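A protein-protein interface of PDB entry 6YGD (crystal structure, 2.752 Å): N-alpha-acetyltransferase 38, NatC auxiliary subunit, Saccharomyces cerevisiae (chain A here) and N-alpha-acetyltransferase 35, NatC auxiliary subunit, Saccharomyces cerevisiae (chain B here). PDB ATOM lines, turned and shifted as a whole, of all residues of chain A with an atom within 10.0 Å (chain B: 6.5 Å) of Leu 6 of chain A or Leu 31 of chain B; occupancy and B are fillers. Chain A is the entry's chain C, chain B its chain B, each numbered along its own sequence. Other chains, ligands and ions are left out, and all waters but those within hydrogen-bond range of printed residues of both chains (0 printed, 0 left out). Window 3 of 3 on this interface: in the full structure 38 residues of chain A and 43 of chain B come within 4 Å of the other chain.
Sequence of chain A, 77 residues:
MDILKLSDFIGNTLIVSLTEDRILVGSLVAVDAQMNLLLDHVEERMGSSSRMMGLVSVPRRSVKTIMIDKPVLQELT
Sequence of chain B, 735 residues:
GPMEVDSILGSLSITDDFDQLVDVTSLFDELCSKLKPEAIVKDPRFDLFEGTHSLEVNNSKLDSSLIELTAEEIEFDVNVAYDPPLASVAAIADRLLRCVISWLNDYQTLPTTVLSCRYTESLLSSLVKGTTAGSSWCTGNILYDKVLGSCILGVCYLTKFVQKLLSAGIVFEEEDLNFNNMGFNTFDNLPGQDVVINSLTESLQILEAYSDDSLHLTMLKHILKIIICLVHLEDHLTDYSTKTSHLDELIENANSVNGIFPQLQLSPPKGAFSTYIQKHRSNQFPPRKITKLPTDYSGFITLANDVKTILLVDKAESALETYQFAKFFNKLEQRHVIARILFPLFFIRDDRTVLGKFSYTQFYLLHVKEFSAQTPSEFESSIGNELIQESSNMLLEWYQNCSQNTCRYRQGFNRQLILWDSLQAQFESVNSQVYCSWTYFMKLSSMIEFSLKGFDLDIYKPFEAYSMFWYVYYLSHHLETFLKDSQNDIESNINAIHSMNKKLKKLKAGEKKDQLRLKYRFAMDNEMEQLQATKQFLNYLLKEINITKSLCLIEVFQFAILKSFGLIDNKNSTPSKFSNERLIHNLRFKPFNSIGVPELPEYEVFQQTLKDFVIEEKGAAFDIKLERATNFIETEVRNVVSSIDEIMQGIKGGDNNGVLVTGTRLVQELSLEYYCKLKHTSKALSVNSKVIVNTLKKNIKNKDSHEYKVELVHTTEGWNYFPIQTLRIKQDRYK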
ATOM      1  N   LYS A   5       9.249  17.269  12.355  1.00  0.00           N
ATOM      2  CA  LYS A   5       8.065  17.872  11.759  1.00  0.00           C
ATOM      3  C   LYS A   5       6.802  17.186  12.240  1.00  0.00           C
ATOM      4  O   LYS A   5       6.836  16.360  13.148  1.00  0.00           O
ATOM      5  CB  LYS A   5       8.132  17.799  10.236  1.00  0.00           C
ATOM      6  CG  LYS A   5       9.475  18.164   9.648  1.00  0.00           C
ATOM      7  CD  LYS A   5       9.381  18.260   8.138  1.00  0.00           C
ATOM      8  CE  LYS A   5       8.418  19.363   7.725  1.00  0.00           C
ATOM      9  NZ  LYS A   5       8.107  19.329   6.270  1.00  0.00           N
ATOM     10  N   LEU A   6       5.677  17.532  11.617  1.00  0.00           N
ATOM     11  CA  LEU A   6       4.453  16.790  11.878  1.00  0.00           C
ATOM     12  C   LEU A   6       4.568  15.351  11.391  1.00  0.00           C
ATOM     13  O   LEU A   6       3.847  14.475  11.878  1.00  0.00           O
ATOM     14  CB  LEU A   6       3.267  17.493  11.216  1.00  0.00           C
ATOM     15  CG  LEU A   6       1.987  17.621  12.041  1.00  0.00           C
ATOM     16  CD1 LEU A   6       2.270  18.172  13.434  1.00  0.00           C
ATOM     17  CD2 LEU A   6       1.011  18.513  11.306  1.00  0.00           C
ATOM     18  N   SER A   7       5.476  15.088  10.446  1.00  0.00           N
ATOM     19  CA  SER A   7       5.637  13.745   9.896  1.00  0.00           C
ATOM     20  C   SER A   7       6.105  12.761  10.960  1.00  0.00           C
ATOM     21  O   SER A   7       5.514  11.689  11.138  1.00  0.00           O
ATOM     22  CB  SER A   7       6.638  13.768   8.738  1.00  0.00           C
ATOM     23  OG  SER A   7       6.278  14.716   7.753  1.00  0.00           O
ATOM     24  N   ASP A   8       7.191  13.104  11.660  1.00  0.00           N
ATOM     25  CA  ASP A   8       7.788  12.186  12.627  1.00  0.00           C
ATOM     26  C   ASP A   8       6.803  11.782  13.722  1.00  0.00           C
ATOM     27  O   ASP A   8       6.918  10.688  14.287  1.00  0.00           O
ATOM     28  CB  ASP A   8       9.047  12.815  13.238  1.00  0.00           C
ATOM     29  CG  ASP A   8       8.768  14.139  13.930  1.00  0.00           C
ATOM     30  OD1 ASP A   8       7.935  14.156  14.858  1.00  0.00           O
ATOM     31  OD2 ASP A   8       9.386  15.161  13.558  1.00  0.00           O
ATOM     32  N   PHE A   9       5.830  12.645  14.036  1.00  0.00           N
ATOM     33  CA  PHE A   9       4.834  12.309  15.053  1.00  0.00           C
ATOM     34  C   PHE A   9       3.984  11.113  14.645  1.00  0.00           C
ATOM     35  O   PHE A   9       3.478  10.390  15.512  1.00  0.00           O
ATOM     36  CB  PHE A   9       3.924  13.508  15.328  1.00  0.00           C
ATOM     37  CG  PHE A   9       4.554  14.571  16.178  1.00  0.00           C
ATOM     38  CD1 PHE A   9       4.551  14.465  17.558  1.00  0.00           C
ATOM     39  CD2 PHE A   9       5.133  15.686  15.598  1.00  0.00           C
ATOM     40  CE1 PHE A   9       5.123  15.445  18.343  1.00  0.00           C
ATOM     41  CE2 PHE A   9       5.706  16.669  16.377  1.00  0.00           C
ATOM     42  CZ  PHE A   9       5.703  16.549  17.752  1.00  0.00           C
ATOM     43  N   ILE A  10       3.808  10.896  13.339  1.00  0.00           N
ATOM     44  CA  ILE A  10       2.963   9.809  12.857  1.00  0.00           C
ATOM     45  C   ILE A  10       3.516   8.472  13.323  1.00  0.00           C
ATOM     46  O   ILE A  10       4.714   8.195  13.190  1.00  0.00           O
ATOM     47  CB  ILE A  10       2.851   9.858  11.327  1.00  0.00           C
ATOM     48  CG1 ILE A  10       2.172  11.156  10.894  1.00  0.00           C
ATOM     49  CG2 ILE A  10       2.080   8.653  10.807  1.00  0.00           C
ATOM     50  CD1 ILE A  10       0.780  11.325  11.461  1.00  0.00           C
ATOM     51  N   GLY A  11       2.639   7.632  13.866  1.00  0.00           N
ATOM     52  CA  GLY A  11       3.040   6.335  14.363  1.00  0.00           C
ATOM     53  C   GLY A  11       3.534   6.328  15.788  1.00  0.00           C
ATOM     54  O   GLY A  11       3.997   5.284  16.260  1.00  0.00           O
ATOM     55  N   ASN A  12       3.448   7.455  16.489  1.00  0.00           N
ATOM     56  CA  ASN A  12       3.921   7.575  17.860  1.00  0.00           C
ATOM     57  C   ASN A  12       2.739   7.856  18.779  1.00  0.00           C
ATOM     58  O   ASN A  12       1.882   8.685  18.458  1.00  0.00           O
ATOM     59  CB  ASN A  12       4.973   8.682  17.978  1.00  0.00           C
ATOM     60  CG  ASN A  12       6.116   8.509  16.989  1.00  0.00           C
ATOM     61  OD1 ASN A  12       6.529   7.389  16.688  1.00  0.00           O
ATOM     62  ND2 ASN A  12       6.627   9.621  16.477  1.00  0.00           N
ATOM     63  N   LEU A  14       0.162   9.152  21.400  1.00  0.00           N
ATOM     64  CA  LEU A  14      -0.179  10.481  21.877  1.00  0.00           C
ATOM     65  C   LEU A  14      -1.365  10.379  22.830  1.00  0.00           C
ATOM     66  O   LEU A  14      -2.105   9.392  22.831  1.00  0.00           O
ATOM     67  CB  LEU A  14      -0.513  11.428  20.715  1.00  0.00           C
ATOM     68  CG  LEU A  14       0.535  11.622  19.619  1.00  0.00           C
ATOM     69  CD1 LEU A  14      -0.034  12.496  18.513  1.00  0.00           C
ATOM     70  CD2 LEU A  14       1.796  12.234  20.182  1.00  0.00           C
ATOM     71  N   LEU A  28      -1.132   8.194  16.698  1.00  0.00           N
ATOM     72  CA  LEU A  28      -1.528   9.081  15.614  1.00  0.00           C
ATOM     73  C   LEU A  28      -1.286   8.420  14.265  1.00  0.00           C
ATOM     74  O   LEU A  28      -0.145   8.105  13.914  1.00  0.00           O
ATOM     75  CB  LEU A  28      -0.751  10.392  15.707  1.00  0.00           C
ATOM     76  CG  LEU A  28      -1.174  11.514  14.761  1.00  0.00           C
ATOM     77  CD1 LEU A  28      -2.566  12.021  15.118  1.00  0.00           C
ATOM     78  CD2 LEU A  28      -0.158  12.645  14.788  1.00  0.00           C
ATOM     79  N   VAL A  29      -2.360   8.211  13.509  1.00  0.00           N
ATOM     80  CA  VAL A  29      -2.240   7.635  12.172  1.00  0.00           C
ATOM     81  C   VAL A  29      -2.083   8.721  11.118  1.00  0.00           C
ATOM     82  O   VAL A  29      -1.258   8.594  10.209  1.00  0.00           O
ATOM     83  CB  VAL A  29      -3.453   6.735  11.865  1.00  0.00           C
ATOM     84  CG1 VAL A  29      -3.225   5.964  10.576  1.00  0.00           C
ATOM     85  CG2 VAL A  29      -3.716   5.788  13.010  1.00  0.00           C
ATOM     86  N   ALA A  30      -2.860   9.800  11.227  1.00  0.00           N
ATOM     87  CA  ALA A  30      -2.836  10.861  10.229  1.00  0.00           C
ATOM     88  C   ALA A  30      -3.336  12.161  10.845  1.00  0.00           C
ATOM     89  O   ALA A  30      -3.981  12.168  11.897  1.00  0.00           O
ATOM     90  CB  ALA A  30      -3.674  10.491   9.000  1.00  0.00           C
ATOM     91  N   VAL A  31      -3.027  13.261  10.162  1.00  0.00           N
ATOM     92  CA  VAL A  31      -3.430  14.607  10.567  1.00  0.00           C
ATOM     93  C   VAL A  31      -3.728  15.402   9.302  1.00  0.00           C
ATOM     94  O   VAL A  31      -2.968  15.340   8.332  1.00  0.00           O
ATOM     95  CB  VAL A  31      -2.329  15.291  11.413  1.00  0.00           C
ATOM     96  CG1 VAL A  31      -2.503  16.802  11.427  1.00  0.00           C
ATOM     97  CG2 VAL A  31      -2.319  14.755  12.830  1.00  0.00           C
ATOM     98  N   ASP A  32      -4.836  16.141   9.299  1.00  0.00           N
ATOM     99  CA  ASP A  32      -5.187  16.990   8.166  1.00  0.00           C
ATOM    100  C   ASP A  32      -4.903  18.456   8.483  1.00  0.00           C
ATOM    101  O   ASP A  32      -4.492  18.815   9.589  1.00  0.00           O
ATOM    102  CB  ASP A  32      -6.655  16.796   7.756  1.00  0.00           C
ATOM    103  CG  ASP A  32      -7.638  17.253   8.820  1.00  0.00           C
ATOM    104  OD1 ASP A  32      -7.209  17.730   9.889  1.00  0.00           O
ATOM    105  OD2 ASP A  32      -8.856  17.131   8.583  1.00  0.00           O
ATOM    106  N   ALA A  33      -5.149  19.309   7.483  1.00  0.00           N
ATOM    107  CA  ALA A  33      -4.838  20.730   7.594  1.00  0.00           C
ATOM    108  C   ALA A  33      -5.630  21.426   8.692  1.00  0.00           C
ATOM    109  O   ALA A  33      -5.178  22.451   9.212  1.00  0.00           O
ATOM    110  CB  ALA A  33      -5.097  21.424   6.263  1.00  0.00           C
ATOM    111  N   GLN A  34      -6.795  20.896   9.056  1.00  0.00           N
ATOM    112  CA  GLN A  34      -7.594  21.468  10.128  1.00  0.00           C
ATOM    113  C   GLN A  34      -7.284  20.841  11.481  1.00  0.00           C
ATOM    114  O   GLN A  34      -8.062  21.015  12.426  1.00  0.00           O
ATOM    115  CB  GLN A  34      -9.086  21.324   9.813  1.00  0.00           C
ATOM    116  CG  GLN A  34      -9.482  21.702   8.390  1.00  0.00           C
ATOM    117  CD  GLN A  34      -9.019  23.089   8.009  1.00  0.00           C
ATOM    118  OE1 GLN A  34      -9.042  24.007   8.827  1.00  0.00           O
ATOM    119  NE2 GLN A  34      -8.578  23.247   6.766  1.00  0.00           N
ATOM    120  N   MET A  35      -6.171  20.110  11.580  1.00  0.00           N
ATOM    121  CA  MET A  35      -5.707  19.433  12.789  1.00  0.00           C
ATOM    122  C   MET A  35      -6.682  18.365  13.287  1.00  0.00           C
ATOM    123  O   MET A  35      -6.668  18.012  14.471  1.00  0.00           O
ATOM    124  CB  MET A  35      -5.390  20.439  13.905  1.00  0.00           C
ATOM    125  CG  MET A  35      -4.387  19.948  14.944  1.00  0.00           C
ATOM    126  SD  MET A  35      -4.288  21.062  16.354  1.00  0.00           S
ATOM    127  CE  MET A  35      -5.970  20.944  16.960  1.00  0.00           C
ATOM    128  N   ASN A  36      -7.531  17.836  12.408  1.00  0.00           N
ATOM    129  CA  ASN A  36      -8.311  16.651  12.742  1.00  0.00           C
ATOM    130  C   ASN A  36      -7.388  15.439  12.811  1.00  0.00           C
ATOM    131  O   ASN A  36      -6.589  15.198  11.902  1.00  0.00           O
ATOM    132  CB  ASN A  36      -9.413  16.414  11.707  1.00  0.00           C
ATOM    133  CG  ASN A  36     -10.413  17.554  11.641  1.00  0.00           C
ATOM    134  OD1 ASN A  36     -10.798  18.116  12.664  1.00  0.00           O
ATOM    135  ND2 ASN A  36     -10.840  17.900  10.430  1.00  0.00           N
ATOM    136  N   LEU A  37      -7.498  14.673  13.896  1.00  0.00           N
ATOM    137  CA  LEU A  37      -6.576  13.582  14.175  1.00  0.00           C
ATOM    138  C   LEU A  37      -7.220  12.234  13.879  1.00  0.00           C
ATOM    139  O   LEU A  37      -8.420  12.045  14.099  1.00  0.00           O
ATOM    140  CB  LEU A  37      -6.113  13.622  15.635  1.00  0.00           C
ATOM    141  CG  LEU A  37      -5.759  14.999  16.199  1.00  0.00           C
ATOM    142  CD1 LEU A  37      -5.504  14.898  17.690  1.00  0.00           C
ATOM    143  CD2 LEU A  37      -4.558  15.597  15.489  1.00  0.00           C
ATOM    144  N   ARG A  60     -11.232  18.837  15.363  1.00  0.00           N
ATOM    145  CA  ARG A  60     -10.481  19.870  16.072  1.00  0.00           C
ATOM    146  C   ARG A  60     -11.261  20.412  17.265  1.00  0.00           C
ATOM    147  O   ARG A  60     -10.698  20.609  18.349  1.00  0.00           O
ATOM    148  CB  ARG A  60     -10.117  21.002  15.111  1.00  0.00           C
ATOM    149  CG  ARG A  60      -9.603  22.257  15.793  1.00  0.00           C
ATOM    150  CD  ARG A  60      -9.421  23.399  14.808  1.00  0.00           C
ATOM    151  NE  ARG A  60      -9.209  24.671  15.496  1.00  0.00           N
ATOM    152  CZ  ARG A  60      -8.022  25.121  15.892  1.00  0.00           C
ATOM    153  NH1 ARG A  60      -6.930  24.402  15.667  1.00  0.00           N
ATOM    154  NH2 ARG A  60      -7.927  26.290  16.513  1.00  0.00           N
ATOM    155  N   ILE A  66      -3.619  18.232  23.817  1.00  0.00           N
ATOM    156  CA  ILE A  66      -2.841  17.174  23.180  1.00  0.00           C
ATOM    157  C   ILE A  66      -1.539  17.036  23.954  1.00  0.00           C
ATOM    158  O   ILE A  66      -0.650  17.890  23.844  1.00  0.00           O
ATOM    159  CB  ILE A  66      -2.561  17.463  21.700  1.00  0.00           C
ATOM    160  CG1 ILE A  66      -3.860  17.440  20.895  1.00  0.00           C
ATOM    161  CG2 ILE A  66      -1.571  16.452  21.136  1.00  0.00           C
ATOM    162  CD1 ILE A  66      -3.657  17.673  19.417  1.00  0.00           C
ATOM    163  N   LEU A  73       8.578  12.054  23.468  1.00  0.00           N
ATOM    164  CA  LEU A  73       8.773  13.293  22.719  1.00  0.00           C
ATOM    165  C   LEU A  73      10.245  13.504  22.389  1.00  0.00           C
ATOM    166  O   LEU A  73      10.601  13.812  21.246  1.00  0.00           O
ATOM    167  CB  LEU A  73       8.224  14.476  23.520  1.00  0.00           C
ATOM    168  CG  LEU A  73       8.356  15.865  22.889  1.00  0.00           C
ATOM    169  CD1 LEU A  73       7.504  15.962  21.634  1.00  0.00           C
ATOM    170  CD2 LEU A  73       7.979  16.951  23.886  1.00  0.00           C
ATOM    171  N   SER B  26      -0.347  23.511  21.494  1.00  0.00           N
ATOM    172  CA  SER B  26       0.089  24.748  20.857  1.00  0.00           C
ATOM    173  C   SER B  26       0.962  24.471  19.639  1.00  0.00           C
ATOM    174  O   SER B  26       0.866  25.174  18.626  1.00  0.00           O
ATOM    175  CB  SER B  26       0.836  25.617  21.868  1.00  0.00           C
ATOM    176  OG  SER B  26       1.386  26.761  21.243  1.00  0.00           O
ATOM    177  N   LEU B  27       1.821  23.452  19.717  1.00  0.00           N
ATOM    178  CA  LEU B  27       2.705  23.143  18.597  1.00  0.00           C
ATOM    179  C   LEU B  27       1.930  22.554  17.426  1.00  0.00           C
ATOM    180  O   LEU B  27       2.215  22.873  16.265  1.00  0.00           O
ATOM    181  CB  LEU B  27       3.808  22.184  19.045  1.00  0.00           C
ATOM    182  CG  LEU B  27       4.751  21.691  17.947  1.00  0.00           C
ATOM    183  CD1 LEU B  27       5.415  22.868  17.252  1.00  0.00           C
ATOM    184  CD2 LEU B  27       5.792  20.741  18.519  1.00  0.00           C
ATOM    185  N   PHE B  28       0.950  21.693  17.708  1.00  0.00           N
ATOM    186  CA  PHE B  28       0.155  21.096  16.640  1.00  0.00           C
ATOM    187  C   PHE B  28      -0.613  22.158  15.864  1.00  0.00           C
ATOM    188  O   PHE B  28      -0.631  22.149  14.628  1.00  0.00           O
ATOM    189  CB  PHE B  28      -0.806  20.055  17.214  1.00  0.00           C
ATOM    190  CG  PHE B  28      -0.303  18.645  17.120  1.00  0.00           C
ATOM    191  CD1 PHE B  28      -0.346  17.959  15.918  1.00  0.00           C
ATOM    192  CD2 PHE B  28       0.201  17.999  18.236  1.00  0.00           C
ATOM    193  CE1 PHE B  28       0.112  16.655  15.830  1.00  0.00           C
ATOM    194  CE2 PHE B  28       0.658  16.697  18.155  1.00  0.00           C
ATOM    195  CZ  PHE B  28       0.614  16.024  16.951  1.00  0.00           C
ATOM    196  N   ASP B  29      -1.259  23.082  16.579  1.00  0.00           N
ATOM    197  CA  ASP B  29      -2.025  24.133  15.917  1.00  0.00           C
ATOM    198  C   ASP B  29      -1.145  24.946  14.976  1.00  0.00           C
ATOM    199  O   ASP B  29      -1.544  25.245  13.843  1.00  0.00           O
ATOM    200  CB  ASP B  29      -2.675  25.039  16.964  1.00  0.00           C
ATOM    201  CG  ASP B  29      -3.772  25.919  16.385  1.00  0.00           C
ATOM    202  OD1 ASP B  29      -3.669  26.321  15.209  1.00  0.00           O
ATOM    203  OD2 ASP B  29      -4.743  26.209  17.113  1.00  0.00           O
ATOM    204  N   GLU B  30       0.059  25.302  15.424  1.00  0.00           N
ATOM    205  CA  GLU B  30       0.924  26.158  14.620  1.00  0.00           C
ATOM    206  C   GLU B  30       1.343  25.471  13.327  1.00  0.00           C
ATOM    207  O   GLU B  30       1.350  26.094  12.258  1.00  0.00           O
ATOM    208  CB  GLU B  30       2.150  26.570  15.432  1.00  0.00           C
ATOM    209  CG  GLU B  30       3.048  27.580  14.739  1.00  0.00           C
ATOM    210  CD  GLU B  30       2.409  28.950  14.617  1.00  0.00           C
ATOM    211  OE1 GLU B  30       1.353  29.184  15.244  1.00  0.00           O
ATOM    212  OE2 GLU B  30       2.966  29.799  13.891  1.00  0.00           O
ATOM    213  N   LEU B  31       1.690  24.186  13.401  1.00  0.00           N
ATOM    214  CA  LEU B  31       2.141  23.479  12.208  1.00  0.00           C
ATOM    215  C   LEU B  31       0.981  23.192  11.259  1.00  0.00           C
ATOM    216  O   LEU B  31       1.138  23.277  10.035  1.00  0.00           O
ATOM    217  CB  LEU B  31       2.856  22.186  12.609  1.00  0.00           C
ATOM    218  CG  LEU B  31       4.055  21.739  11.763  1.00  0.00           C
ATOM    219  CD1 LEU B  31       4.852  20.654  12.478  1.00  0.00           C
ATOM    220  CD2 LEU B  31       3.613  21.261  10.385  1.00  0.00           C
ATOM    221  N   CYS B  32      -0.193  22.864  11.803  1.00  0.00           N
ATOM    222  CA  CYS B  32      -1.334  22.519  10.957  1.00  0.00           C
ATOM    223  C   CYS B  32      -1.892  23.741  10.240  1.00  0.00           C
ATOM    224  O   CYS B  32      -2.396  23.628   9.116  1.00  0.00           O
ATOM    225  CB  CYS B  32      -2.426  21.848  11.789  1.00  0.00           C
ATOM    226  SG  CYS B  32      -1.976  20.225  12.425  1.00  0.00           S
ATOM    227  N   SER B  33      -1.832  24.912  10.878  1.00  0.00           N
ATOM    228  CA  SER B  33      -2.247  26.136  10.201  1.00  0.00           C
ATOM    229  C   SER B  33      -1.359  26.415   8.996  1.00  0.00           C
ATOM    230  O   SER B  33      -1.843  26.837   7.939  1.00  0.00           O
ATOM    231  CB  SER B  33      -2.217  27.314  11.177  1.00  0.00           C
ATOM    232  OG  SER B  33      -3.025  27.067  12.314  1.00  0.00           O
ATOM    233  N   LYS B  34      -0.055  26.163   9.136  1.00  0.00           N
ATOM    234  CA  LYS B  34       0.893  26.393   8.051  1.00  0.00           C
ATOM    235  C   LYS B  34       0.622  25.488   6.856  1.00  0.00           C
ATOM    236  O   LYS B  34       0.808  25.903   5.706  1.00  0.00           O
ATOM    237  CB  LYS B  34       2.320  26.182   8.565  1.00  0.00           C
ATOM    238  CG  LYS B  34       3.331  25.765   7.507  1.00  0.00           C
ATOM    239  CD  LYS B  34       4.627  25.288   8.147  1.00  0.00           C
ATOM    240  CE  LYS B  34       5.592  24.739   7.108  1.00  0.00           C
ATOM    241  NZ  LYS B  34       6.824  24.198   7.749  1.00  0.00           N
ATOM    242  N   LEU B  35       0.169  24.265   7.104  1.00  0.00           N
ATOM    243  CA  LEU B  35       0.029  23.276   6.046  1.00  0.00           C
ATOM    244  C   LEU B  35      -1.116  23.627   5.097  1.00  0.00           C
ATOM    245  O   LEU B  35      -2.082  24.299   5.468  1.00  0.00           O
ATOM    246  CB  LEU B  35      -0.194  21.896   6.657  1.00  0.00           C
ATOM    247  CG  LEU B  35      -0.047  20.688   5.736  1.00  0.00           C
ATOM    248  CD1 LEU B  35       1.238  20.784   4.939  1.00  0.00           C
ATOM    249  CD2 LEU B  35      -0.070  19.420   6.562  1.00  0.00           C
ATOM    250  N   VAL B  41      -1.088  14.667   6.460  1.00  0.00           N
ATOM    251  CA  VAL B  41       0.126  14.087   7.020  1.00  0.00           C
ATOM    252  C   VAL B  41      -0.184  12.661   7.454  1.00  0.00           C
ATOM    253  O   VAL B  41      -0.978  12.439   8.369  1.00  0.00           O
ATOM    254  CB  VAL B  41       0.668  14.911   8.190  1.00  0.00           C
ATOM    255  CG1 VAL B  41       1.787  14.144   8.873  1.00  0.00           C
ATOM    256  CG2 VAL B  41       1.176  16.246   7.693  1.00  0.00           C
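The side-chain sulfur (SD) of Met 35 of chain A lies within hydrogen-bond range of the backbone NH (N) of Asp 29 of chain B (3.6 Å). The backbone carbonyl oxygen (O) of Val 31 of chain A is in hydrogen-bond range of the backbone NH (N) of Val 41 of chain B (2.7 Å). The backbone carbonyl oxygen (O) of Ala 33 of chain A lies close to the backbone carbonyl oxygen (O) of Cys 32 of chain B (3.0 Å). NH1 of Arg 60 of chain A is in salt-bridge range of OD2 of Asp 29 of chain B, at 3.2 Å.
The backbone NH (N) of Arg 60 of chain A sits at hydrogen-bond distance from the side-chain amide oxygen (OD1) of Asn 36 of chain A. The backbone NH of Met 35 of chain A lies within hydrogen-bond range of the side-chain carboxylate of Asp 32 of chain A, at 3.1 Å. The side-chain carboxylate (OD2) of Asp 8 of chain A is in hydrogen-bond range of the backbone NH (N) of Lys 5 of chain A. The backbone carbonyl oxygen (O) of Phe 28 of chain B lies within hydrogen-bond range of the side-chain sulfur (SG) of Cys 32 of chain B, at 3.2 Å. The side-chain hydroxyl (OG) of Ser 33 of chain B is in hydrogen-bond range of the backbone carbonyl oxygen (O) of Asp 29 of chain B (2.8 Å).
Among the printed residues, pairs that only touch across the chains: Ala 30 of chain A with Val 41 of chain B, Leu 6 of chain A with Leu 31 of chain B, Met 35 of chain A with Cys 32 of chain B, Leu 6 of chain A with Phe 28 of chain B, Val 31 of chain A with Cys 32 of chain B, Leu 6 of chain A with Cys 32 of chain B, Ile 10 of chain A with Val 41 of chain B, Leu 6 of chain A with Val 41 of chain B, Met 35 of chain A with Phe 28 of chain B, Ile 66 of chain A with Phe 28 of chain B, Leu 14 of chain A with Phe 28 of chain B and Lys 5 of chain A with Leu 31 of chain B.
Of chain B, only Phe 28, Leu 31, Cys 32 and Val 41 come within 4 Å of Leu 6 of chain A. Of the printed residues of chain A, Leu 31 of chain B touches Lys 5 (3.99 Å) and Leu 6 (3.3 Å). Of chain A, only Leu 6, Leu 14, Met 35 and Ile 66 come within 4 Å of Phe 28 of chain B. No residue of chain A comes within 4 Å of Ser 33 of chain B. No residue of chain A comes within 4 Å of Leu 35 of chain B. Printed residues of chain B within 4 Å of Ile 66 of chain A: Phe 28 (3.7 Å). Of the printed residues of chain B, Ile 10 of chain A touches Val 41. Printed residues of chain A within 4 Å of Asp 29 of chain B: Met 35 (3.6 Å) and Arg 60 (3.2 Å). Of the printed residues of chain B, Met 35 of chain A touches Phe 28 (3.7 Å), Asp 29 (3.6 Å) and Cys 32 (3.5 Å). Leu 37 of chain A touches none of the printed residues of chain B. The nearest printed residue of chain B that does not touch Ala 30 of chain A is Phe 28 of chain B (7.2 Å).
Hydrophobic or aromatic side chains of chain A within 4 Å of the printed part of chain B: Leu 6, Ile 10, Leu 14, Ala 30, Val 31, Met 35 and Ile 66. Of the 11 printed residues of chain B, 5 touch a printed residue of chain A. Printed residues of chain B that touch a printed residue of chain A: Phe 28, Asp 29, Leu 31, Cys 32 and Val 41. Hydrophobic or aromatic side chains of chain B within 4 Å of the printed part of chain A: Phe 28, Leu 31 and Val 41.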
